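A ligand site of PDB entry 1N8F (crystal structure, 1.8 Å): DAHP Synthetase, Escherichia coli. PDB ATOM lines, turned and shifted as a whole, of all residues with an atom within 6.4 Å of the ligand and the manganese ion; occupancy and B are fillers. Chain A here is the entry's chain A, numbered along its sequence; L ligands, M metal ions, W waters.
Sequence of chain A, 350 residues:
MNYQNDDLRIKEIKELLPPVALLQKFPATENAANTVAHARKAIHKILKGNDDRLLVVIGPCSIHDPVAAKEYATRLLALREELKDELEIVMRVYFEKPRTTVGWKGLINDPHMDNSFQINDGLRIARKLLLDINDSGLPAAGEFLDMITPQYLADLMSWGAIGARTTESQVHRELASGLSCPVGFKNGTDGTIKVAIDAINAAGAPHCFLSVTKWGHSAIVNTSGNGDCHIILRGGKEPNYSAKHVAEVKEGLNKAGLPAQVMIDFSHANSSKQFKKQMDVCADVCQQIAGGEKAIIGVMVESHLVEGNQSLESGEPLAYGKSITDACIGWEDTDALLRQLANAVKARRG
The manganese ion is bound by OE2 of Glu 302 (2.1 Å), OD2 of Asp 326 (2.1 Å), water W4 (2.4 Å), NE2 of His 268 (2.4 Å) and SG of Cys 61 (2.6 Å).
The manganese ion has five donor atoms within binding distance.
A ring nitrogen (NE2) of His 268 lies close to an oxygen (O1) of the ligand, 3.3 Å away.
The guanidinium group (NE) of Arg 234 is in salt-bridge range of an oxygen (O6) of the ligand, 2.7 Å away.
NZ of Lys 97 lies within salt-bridge range of O1 of the ligand, at 2.8 Å.
The side-chain amino group of Lys 186 lies within salt-bridge range of an oxygen (O6) of the ligand, 2.8 Å away.
The guanidinium group of Arg 92 lies within salt-bridge range of an oxygen (O1) of the ligand, 2.8 Å away.
NH1 of Arg 165 is in salt-bridge range of O5 of the ligand, at 2.9 Å.
N of Ala 164 is in hydrogen-bond range of O4 of the ligand.
Water W4 lies within hydrogen-bond range of NZ of Lys 97 (2.8 Å) and O1 of the ligand (2.8 Å).
Water W5 lies within hydrogen-bond range of an oxygen (O2) of the ligand (2.6 Å) and the side-chain hydroxyl of Tyr 94 (2.7 Å).
Water W6 lies within hydrogen-bond range of O5 of the ligand (2.7 Å), NH2 of Arg 165 (3.0 Å) and NH2 of Arg 234 (3.2 Å).
Water W2 lies within hydrogen-bond range of NH1 of Arg 165 (2.8 Å), O4 of the ligand (2.8 Å) and N of Ala 164 (3.2 Å).
Water W3 bridges the side-chain carboxylate (OE1) of Glu 143 (2.8 Å) and an oxygen (O4) of the ligand (3.0 Å).
The side-chain carboxylate (OE1) of Glu 302 lies within hydrogen-bond range of the side-chain hydroxyl (OG) of Ser 267, at 2.6 Å.
ND1 of His 268 sits at hydrogen-bond distance from OD2 of Asp 265, 2.7 Å away.
O of Cys 61 is in hydrogen-bond range of NZ of Lys 97, at 2.8 Å.
OG1 of Thr 325 sits close to SG of Cys 61, 3.0 Å away.
The side-chain carboxylate (OD2) of Asp 265 lies within salt-bridge range of the side-chain amino group (NZ) of Lys 186 (2.8 Å).
N of Lys 186 is in hydrogen-bond range of O of Ile 162 (3.2 Å).
The guanidinium group of Arg 92 is in hydrogen-bond range of the side-chain sulfur of Met 300, at 3.4 Å.
The backbone carbonyl oxygen (O) of Pro 60 is in hydrogen-bond range of the guanidinium group (NE) of Arg 92.
Lys 97 touches the manganese ion (NZ to MN, 3.996 Å).
Within 4 Å of the manganese ion: Cys 61, Lys 97, His 268, Glu 302 and Asp 326.
Residues that only touch the ligand: Gly 163, Glu 143, Pro 98 and Tyr 94.
Within 4 Å of the ligand: Arg 92, Tyr 94, Lys 97, Pro 98, Glu 143, Gly 163, Ala 164, Arg 165, Lys 186, Arg 234, His 268 and Glu 302.
Along chain A the residues within 4 Å of the ligand span positions 92 to 302.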
ATOM      1  N   PRO A  60      16.786  -7.302  20.018  1.00  0.00           N
ATOM      2  CA  PRO A  60      17.818  -6.279  19.822  1.00  0.00           C
ATOM      3  C   PRO A  60      17.238  -4.885  19.573  1.00  0.00           C
ATOM      4  O   PRO A  60      16.105  -4.742  19.111  1.00  0.00           O
ATOM      5  CB  PRO A  60      18.579  -6.786  18.598  1.00  0.00           C
ATOM      6  CG  PRO A  60      18.437  -8.280  18.721  1.00  0.00           C
ATOM      7  CD  PRO A  60      16.988  -8.432  19.092  1.00  0.00           C
ATOM      8  N   CYS A  61      18.025  -3.865  19.899  1.00  0.00           N
ATOM      9  CA  CYS A  61      17.609  -2.494  19.667  1.00  0.00           C
ATOM     10  C   CYS A  61      17.523  -2.358  18.150  1.00  0.00           C
ATOM     11  O   CYS A  61      16.617  -1.718  17.617  1.00  0.00           O
ATOM     12  CB  CYS A  61      18.649  -1.511  20.207  1.00  0.00           C
ATOM     13  SG  CYS A  61      18.381   0.195  19.650  1.00  0.00           S
ATOM     14  N   SER A  62      18.478  -2.989  17.477  1.00  0.00           N
ATOM     15  CA  SER A  62      18.541  -2.972  16.013  1.00  0.00           C
ATOM     16  C   SER A  62      19.210  -4.224  15.484  1.00  0.00           C
ATOM     17  O   SER A  62      20.054  -4.818  16.162  1.00  0.00           O
ATOM     18  CB  SER A  62      19.325  -1.755  15.522  1.00  0.00           C
ATOM     19  OG  SER A  62      20.687  -1.830  15.914  1.00  0.00           O
ATOM     20  N   ARG A  92      11.776  -8.360  18.487  1.00  0.00           N
ATOM     21  CA  ARG A  92      12.045  -7.034  17.945  1.00  0.00           C
ATOM     22  C   ARG A  92      12.979  -7.281  16.768  1.00  0.00           C
ATOM     23  O   ARG A  92      14.116  -7.716  16.956  1.00  0.00           O
ATOM     24  CB  ARG A  92      12.776  -6.151  18.971  1.00  0.00           C
ATOM     25  CG  ARG A  92      11.904  -5.468  20.003  1.00  0.00           C
ATOM     26  CD  ARG A  92      12.758  -4.596  20.921  1.00  0.00           C
ATOM     27  NE  ARG A  92      13.572  -3.647  20.166  1.00  0.00           N
ATOM     28  CZ  ARG A  92      13.405  -2.335  20.182  1.00  0.00           C
ATOM     29  NH1 ARG A  92      12.449  -1.774  20.910  1.00  0.00           N
ATOM     30  NH2 ARG A  92      14.197  -1.568  19.447  1.00  0.00           N
ATOM     31  N   TYR A  94      14.005  -4.884  14.315  1.00  0.00           N
ATOM     32  CA  TYR A  94      14.096  -3.495  13.860  1.00  0.00           C
ATOM     33  C   TYR A  94      15.130  -3.208  12.788  1.00  0.00           C
ATOM     34  O   TYR A  94      16.337  -3.242  13.048  1.00  0.00           O
ATOM     35  CB  TYR A  94      14.333  -2.587  15.062  1.00  0.00           C
ATOM     36  CG  TYR A  94      13.098  -2.351  15.920  1.00  0.00           C
ATOM     37  CD1 TYR A  94      12.307  -3.420  16.340  1.00  0.00           C
ATOM     38  CD2 TYR A  94      12.743  -1.059  16.318  1.00  0.00           C
ATOM     39  CE1 TYR A  94      11.176  -3.198  17.139  1.00  0.00           C
ATOM     40  CE2 TYR A  94      11.624  -0.837  17.109  1.00  0.00           C
ATOM     41  CZ  TYR A  94      10.845  -1.907  17.520  1.00  0.00           C
ATOM     42  OH  TYR A  94       9.738  -1.686  18.304  1.00  0.00           O
ATOM     43  N   GLU A  96      14.887  -0.237  10.914  1.00  0.00           N
ATOM     44  CA  GLU A  96      14.950   1.211  10.753  1.00  0.00           C
ATOM     45  C   GLU A  96      15.124   1.927  12.093  1.00  0.00           C
ATOM     46  O   GLU A  96      14.352   1.706  13.029  1.00  0.00           O
ATOM     47  CB  GLU A  96      13.680   1.713  10.059  1.00  0.00           C
ATOM     48  CG  GLU A  96      13.246   0.866   8.889  1.00  0.00           C
ATOM     49  CD  GLU A  96      12.247   1.552   7.976  1.00  0.00           C
ATOM     50  OE1 GLU A  96      11.223   2.079   8.478  1.00  0.00           O
ATOM     51  OE2 GLU A  96      12.486   1.551   6.747  1.00  0.00           O
ATOM     52  N   LYS A  97      16.117   2.809  12.166  1.00  0.00           N
ATOM     53  CA  LYS A  97      16.400   3.543  13.400  1.00  0.00           C
ATOM     54  C   LYS A  97      16.377   5.062  13.270  1.00  0.00           C
ATOM     55  O   LYS A  97      17.067   5.643  12.426  1.00  0.00           O
ATOM     56  CB  LYS A  97      17.782   3.118  13.925  1.00  0.00           C
ATOM     57  CG  LYS A  97      17.961   1.610  14.094  1.00  0.00           C
ATOM     58  CD  LYS A  97      16.910   1.023  15.013  1.00  0.00           C
ATOM     59  CE  LYS A  97      17.042   1.557  16.431  1.00  0.00           C
ATOM     60  NZ  LYS A  97      15.981   1.014  17.318  1.00  0.00           N
ATOM     61  N   PRO A  98      15.579   5.735  14.123  1.00  0.00           N
ATOM     62  CA  PRO A  98      15.472   7.197  14.101  1.00  0.00           C
ATOM     63  C   PRO A  98      16.612   7.744  14.962  1.00  0.00           C
ATOM     64  O   PRO A  98      16.820   7.278  16.079  1.00  0.00           O
ATOM     65  CB  PRO A  98      14.111   7.446  14.735  1.00  0.00           C
ATOM     66  CG  PRO A  98      14.049   6.377  15.778  1.00  0.00           C
ATOM     67  CD  PRO A  98      14.579   5.152  15.040  1.00  0.00           C
ATOM     68  N   GLU A 143       9.808  -0.953  13.984  1.00  0.00           N
ATOM     69  CA  GLU A 143       9.320   0.417  13.925  1.00  0.00           C
ATOM     70  C   GLU A 143       9.071   0.779  12.477  1.00  0.00           C
ATOM     71  O   GLU A 143       9.902   0.526  11.603  1.00  0.00           O
ATOM     72  CB  GLU A 143      10.321   1.424  14.494  1.00  0.00           C
ATOM     73  CG  GLU A 143       9.772   2.871  14.438  1.00  0.00           C
ATOM     74  CD  GLU A 143      10.758   3.942  14.877  1.00  0.00           C
ATOM     75  OE1 GLU A 143      11.626   3.643  15.732  1.00  0.00           O
ATOM     76  OE2 GLU A 143      10.640   5.089  14.385  1.00  0.00           O
ATOM     77  N   ALA A 161       5.521  -0.377  15.597  1.00  0.00           N
ATOM     78  CA  ALA A 161       5.646   0.742  16.528  1.00  0.00           C
ATOM     79  C   ALA A 161       5.937   2.034  15.768  1.00  0.00           C
ATOM     80  O   ALA A 161       6.621   2.023  14.746  1.00  0.00           O
ATOM     81  CB  ALA A 161       6.773   0.465  17.524  1.00  0.00           C
ATOM     82  N   ILE A 162       5.392   3.129  16.280  1.00  0.00           N
ATOM     83  CA  ILE A 162       5.636   4.437  15.715  1.00  0.00           C
ATOM     84  C   ILE A 162       6.470   5.057  16.811  1.00  0.00           C
ATOM     85  O   ILE A 162       6.027   5.158  17.969  1.00  0.00           O
ATOM     86  CB  ILE A 162       4.334   5.252  15.504  1.00  0.00           C
ATOM     87  CG1 ILE A 162       3.449   4.575  14.449  1.00  0.00           C
ATOM     88  CG2 ILE A 162       4.676   6.675  15.051  1.00  0.00           C
ATOM     89  CD1 ILE A 162       4.122   4.364  13.110  1.00  0.00           C
ATOM     90  N   GLY A 163       7.700   5.451  16.464  1.00  0.00           N
ATOM     91  CA  GLY A 163       8.611   6.023  17.441  1.00  0.00           C
ATOM     92  C   GLY A 163       8.185   7.300  18.138  1.00  0.00           C
ATOM     93  O   GLY A 163       7.310   8.025  17.657  1.00  0.00           O
ATOM     94  N   ALA A 164       8.810   7.571  19.270  1.00  0.00           N
ATOM     95  CA  ALA A 164       8.513   8.765  20.051  1.00  0.00           C
ATOM     96  C   ALA A 164       8.672  10.044  19.236  1.00  0.00           C
ATOM     97  O   ALA A 164       7.912  10.994  19.389  1.00  0.00           O
ATOM     98  CB  ALA A 164       9.424   8.815  21.283  1.00  0.00           C
ATOM     99  N   ARG A 165       9.658  10.046  18.344  1.00  0.00           N
ATOM    100  CA  ARG A 165       9.944  11.222  17.522  1.00  0.00           C
ATOM    101  C   ARG A 165       9.007  11.394  16.336  1.00  0.00           C
ATOM    102  O   ARG A 165       9.075  12.412  15.635  1.00  0.00           O
ATOM    103  CB  ARG A 165      11.390  11.153  17.027  1.00  0.00           C
ATOM    104  CG  ARG A 165      12.379  11.038  18.171  1.00  0.00           C
ATOM    105  CD  ARG A 165      13.804  10.805  17.683  1.00  0.00           C
ATOM    106  NE  ARG A 165      14.691  10.608  18.822  1.00  0.00           N
ATOM    107  CZ  ARG A 165      14.712   9.519  19.585  1.00  0.00           C
ATOM    108  NH1 ARG A 165      13.878   8.513  19.341  1.00  0.00           N
ATOM    109  NH2 ARG A 165      15.541   9.448  20.616  1.00  0.00           N
ATOM    110  N   LYS A 186       4.438   5.397  20.707  1.00  0.00           N
ATOM    111  CA  LYS A 186       5.238   5.808  21.848  1.00  0.00           C
ATOM    112  C   LYS A 186       4.926   7.240  22.258  1.00  0.00           C
ATOM    113  O   LYS A 186       4.592   8.071  21.419  1.00  0.00           O
ATOM    114  CB  LYS A 186       6.716   5.673  21.517  1.00  0.00           C
ATOM    115  CG  LYS A 186       7.142   4.228  21.340  1.00  0.00           C
ATOM    116  CD  LYS A 186       8.627   4.099  21.424  1.00  0.00           C
ATOM    117  CE  LYS A 186       9.021   2.737  21.951  1.00  0.00           C
ATOM    118  NZ  LYS A 186      10.464   2.740  22.293  1.00  0.00           N
ATOM    119  N   ASN A 187       5.008   7.520  23.560  1.00  0.00           N
ATOM    120  CA  ASN A 187       4.769   8.885  24.008  1.00  0.00           C
ATOM    121  C   ASN A 187       5.978   9.702  23.534  1.00  0.00           C
ATOM    122  O   ASN A 187       6.985   9.127  23.110  1.00  0.00           O
ATOM    123  CB  ASN A 187       4.602   8.954  25.538  1.00  0.00           C
ATOM    124  CG  ASN A 187       5.844   8.485  26.304  1.00  0.00           C
ATOM    125  OD1 ASN A 187       5.848   7.396  26.876  1.00  0.00           O
ATOM    126  ND2 ASN A 187       6.874   9.308  26.322  1.00  0.00           N
ATOM    127  N   THR A 189       9.349  12.150  23.286  1.00  0.00           N
ATOM    128  CA  THR A 189      10.655  12.065  23.948  1.00  0.00           C
ATOM    129  C   THR A 189      10.745  12.920  25.204  1.00  0.00           C
ATOM    130  O   THR A 189      11.603  12.703  26.061  1.00  0.00           O
ATOM    131  CB  THR A 189      11.794  12.479  22.998  1.00  0.00           C
ATOM    132  OG1 THR A 189      11.526  13.776  22.447  1.00  0.00           O
ATOM    133  CG2 THR A 189      11.948  11.465  21.864  1.00  0.00           C
ATOM    134  N   ARG A 234       7.384   4.964  27.257  1.00  0.00           N
ATOM    135  CA  ARG A 234       8.829   4.789  27.134  1.00  0.00           C
ATOM    136  C   ARG A 234       9.617   5.856  27.887  1.00  0.00           C
ATOM    137  O   ARG A 234      10.802   6.070  27.628  1.00  0.00           O
ATOM    138  CB  ARG A 234       9.237   4.771  25.653  1.00  0.00           C
ATOM    139  CG  ARG A 234       8.682   5.918  24.802  1.00  0.00           C
ATOM    140  CD  ARG A 234       9.485   7.202  24.967  1.00  0.00           C
ATOM    141  NE  ARG A 234      10.781   7.123  24.288  1.00  0.00           N
ATOM    142  CZ  ARG A 234      11.786   7.962  24.495  1.00  0.00           C
ATOM    143  NH1 ARG A 234      11.662   8.944  25.372  1.00  0.00           N
ATOM    144  NH2 ARG A 234      12.915   7.836  23.812  1.00  0.00           N
ATOM    145  N   ASP A 265       7.488   0.166  27.854  1.00  0.00           N
ATOM    146  CA  ASP A 265       8.822  -0.095  27.321  1.00  0.00           C
ATOM    147  C   ASP A 265       9.753   0.003  28.527  1.00  0.00           C
ATOM    148  O   ASP A 265       9.769   1.021  29.218  1.00  0.00           O
ATOM    149  CB  ASP A 265       9.179   0.981  26.284  1.00  0.00           C
ATOM    150  CG  ASP A 265      10.580   0.828  25.702  1.00  0.00           C
ATOM    151  OD1 ASP A 265      11.311  -0.101  26.100  1.00  0.00           O
ATOM    152  OD2 ASP A 265      10.947   1.654  24.840  1.00  0.00           O
ATOM    153  N   SER A 267      12.988  -0.125  28.372  1.00  0.00           N
ATOM    154  CA  SER A 267      14.220   0.522  27.956  1.00  0.00           C
ATOM    155  C   SER A 267      14.112   2.023  27.678  1.00  0.00           C
ATOM    156  O   SER A 267      13.173   2.689  28.119  1.00  0.00           O
ATOM    157  CB  SER A 267      14.792  -0.206  26.737  1.00  0.00           C
ATOM    158  OG  SER A 267      16.187   0.051  26.595  1.00  0.00           O
ATOM    159  N   HIS A 268      15.091   2.528  26.937  1.00  0.00           N
ATOM    160  CA  HIS A 268      15.175   3.935  26.570  1.00  0.00           C
ATOM    161  C   HIS A 268      15.061   4.864  27.771  1.00  0.00           C
ATOM    162  O   HIS A 268      15.862   4.749  28.701  1.00  0.00           O
ATOM    163  CB  HIS A 268      14.127   4.255  25.499  1.00  0.00           C
ATOM    164  CG  HIS A 268      14.215   3.357  24.309  1.00  0.00           C
ATOM    165  ND1 HIS A 268      13.459   2.218  24.178  1.00  0.00           N
ATOM    166  CD2 HIS A 268      15.057   3.372  23.240  1.00  0.00           C
ATOM    167  CE1 HIS A 268      13.826   1.561  23.091  1.00  0.00           C
ATOM    168  NE2 HIS A 268      14.794   2.252  22.509  1.00  0.00           N
ATOM    169  N   MET A 300       7.910  -3.964  26.416  1.00  0.00           N
ATOM    170  CA  MET A 300       8.928  -3.945  25.392  1.00  0.00           C
ATOM    171  C   MET A 300      10.264  -4.008  26.098  1.00  0.00           C
ATOM    172  O   MET A 300      10.475  -3.313  27.077  1.00  0.00           O
ATOM    173  CB  MET A 300       8.830  -2.658  24.576  1.00  0.00           C
ATOM    174  CG  MET A 300       9.904  -2.484  23.534  1.00  0.00           C
ATOM    175  SD  MET A 300       9.627  -0.974  22.587  1.00  0.00           S
ATOM    176  CE  MET A 300       8.401  -1.550  21.424  1.00  0.00           C
ATOM    177  N   GLU A 302      14.705  -4.429  25.411  1.00  0.00           N
ATOM    178  CA  GLU A 302      15.825  -4.481  24.494  1.00  0.00           C
ATOM    179  C   GLU A 302      16.773  -5.529  25.021  1.00  0.00           C
ATOM    180  O   GLU A 302      17.406  -5.366  26.071  1.00  0.00           O
ATOM    181  CB  GLU A 302      16.502  -3.111  24.389  1.00  0.00           C
ATOM    182  CG  GLU A 302      15.600  -2.097  23.681  1.00  0.00           C
ATOM    183  CD  GLU A 302      16.323  -0.848  23.224  1.00  0.00           C
ATOM    184  OE1 GLU A 302      16.882  -0.130  24.070  1.00  0.00           O
ATOM    185  OE2 GLU A 302      16.321  -0.579  22.009  1.00  0.00           O
ATOM    186  N   THR A 325      23.770  -0.250  18.597  1.00  0.00           N
ATOM    187  CA  THR A 325      22.972   0.936  18.915  1.00  0.00           C
ATOM    188  C   THR A 325      22.750   0.977  20.430  1.00  0.00           C
ATOM    189  O   THR A 325      23.734   1.055  21.173  1.00  0.00           O
ATOM    190  CB  THR A 325      21.621   0.955  18.152  1.00  0.00           C
ATOM    191  OG1 THR A 325      20.980  -0.326  18.227  1.00  0.00           O
ATOM    192  CG2 THR A 325      21.859   1.304  16.680  1.00  0.00           C
ATOM    193  N   ASP A 326      21.509   0.905  20.900  1.00  0.00           N
ATOM    194  CA  ASP A 326      21.278   0.952  22.349  1.00  0.00           C
ATOM    195  C   ASP A 326      21.730  -0.316  23.057  1.00  0.00           C
ATOM    196  O   ASP A 326      21.650  -1.415  22.494  1.00  0.00           O
ATOM    197  CB  ASP A 326      19.805   1.192  22.692  1.00  0.00           C
ATOM    198  CG  ASP A 326      19.326   2.573  22.290  1.00  0.00           C
ATOM    199  OD1 ASP A 326      20.152   3.514  22.275  1.00  0.00           O
ATOM    200  OD2 ASP A 326      18.118   2.718  22.019  1.00  0.00           O
HETATM  201  C1  LIG L   1      13.065   1.832  19.803  1.00  0.00           C
HETATM  202  O1  LIG L   1      14.148   1.277  19.391  1.00  0.00           O
HETATM  203  O2  LIG L   1      12.156   1.208  20.290  1.00  0.00           O
HETATM  204  C2  LIG L   1      13.037   3.344  19.643  1.00  0.00           C
HETATM  205  C3  LIG L   1      13.531   4.109  18.630  1.00  0.00           C
HETATM  206  O3  LIG L   1      12.436   3.982  20.739  1.00  0.00           O
HETATM  207  P1  LIG L   1      11.941   5.492  20.910  1.00  0.00           P
HETATM  208  O4  LIG L   1      11.066   5.814  19.676  1.00  0.00           O
HETATM  209  O5  LIG L   1      13.205   6.291  21.011  1.00  0.00           O
HETATM  210  O6  LIG L   1      11.071   5.513  22.112  1.00  0.00           O
HETATM  211 MN    MN M   1      16.665   1.361  21.240  1.00  0.00          MN
HETATM  212  O   HOH W   1      16.134   5.460  20.078  1.00  0.00           O
HETATM  213  O   HOH W   2      11.621   7.863  17.870  1.00  0.00           O
HETATM  214  O   HOH W   3      10.263   3.315  18.167  1.00  0.00           O
HETATM  215  O   HOH W   4      16.500   2.838  19.398  1.00  0.00           O
HETATM  216  O   HOH W   5       9.770   0.910  19.183  1.00  0.00           O
HETATM  217  O   HOH W   6      15.544   6.904  22.277  1.00  0.00           O
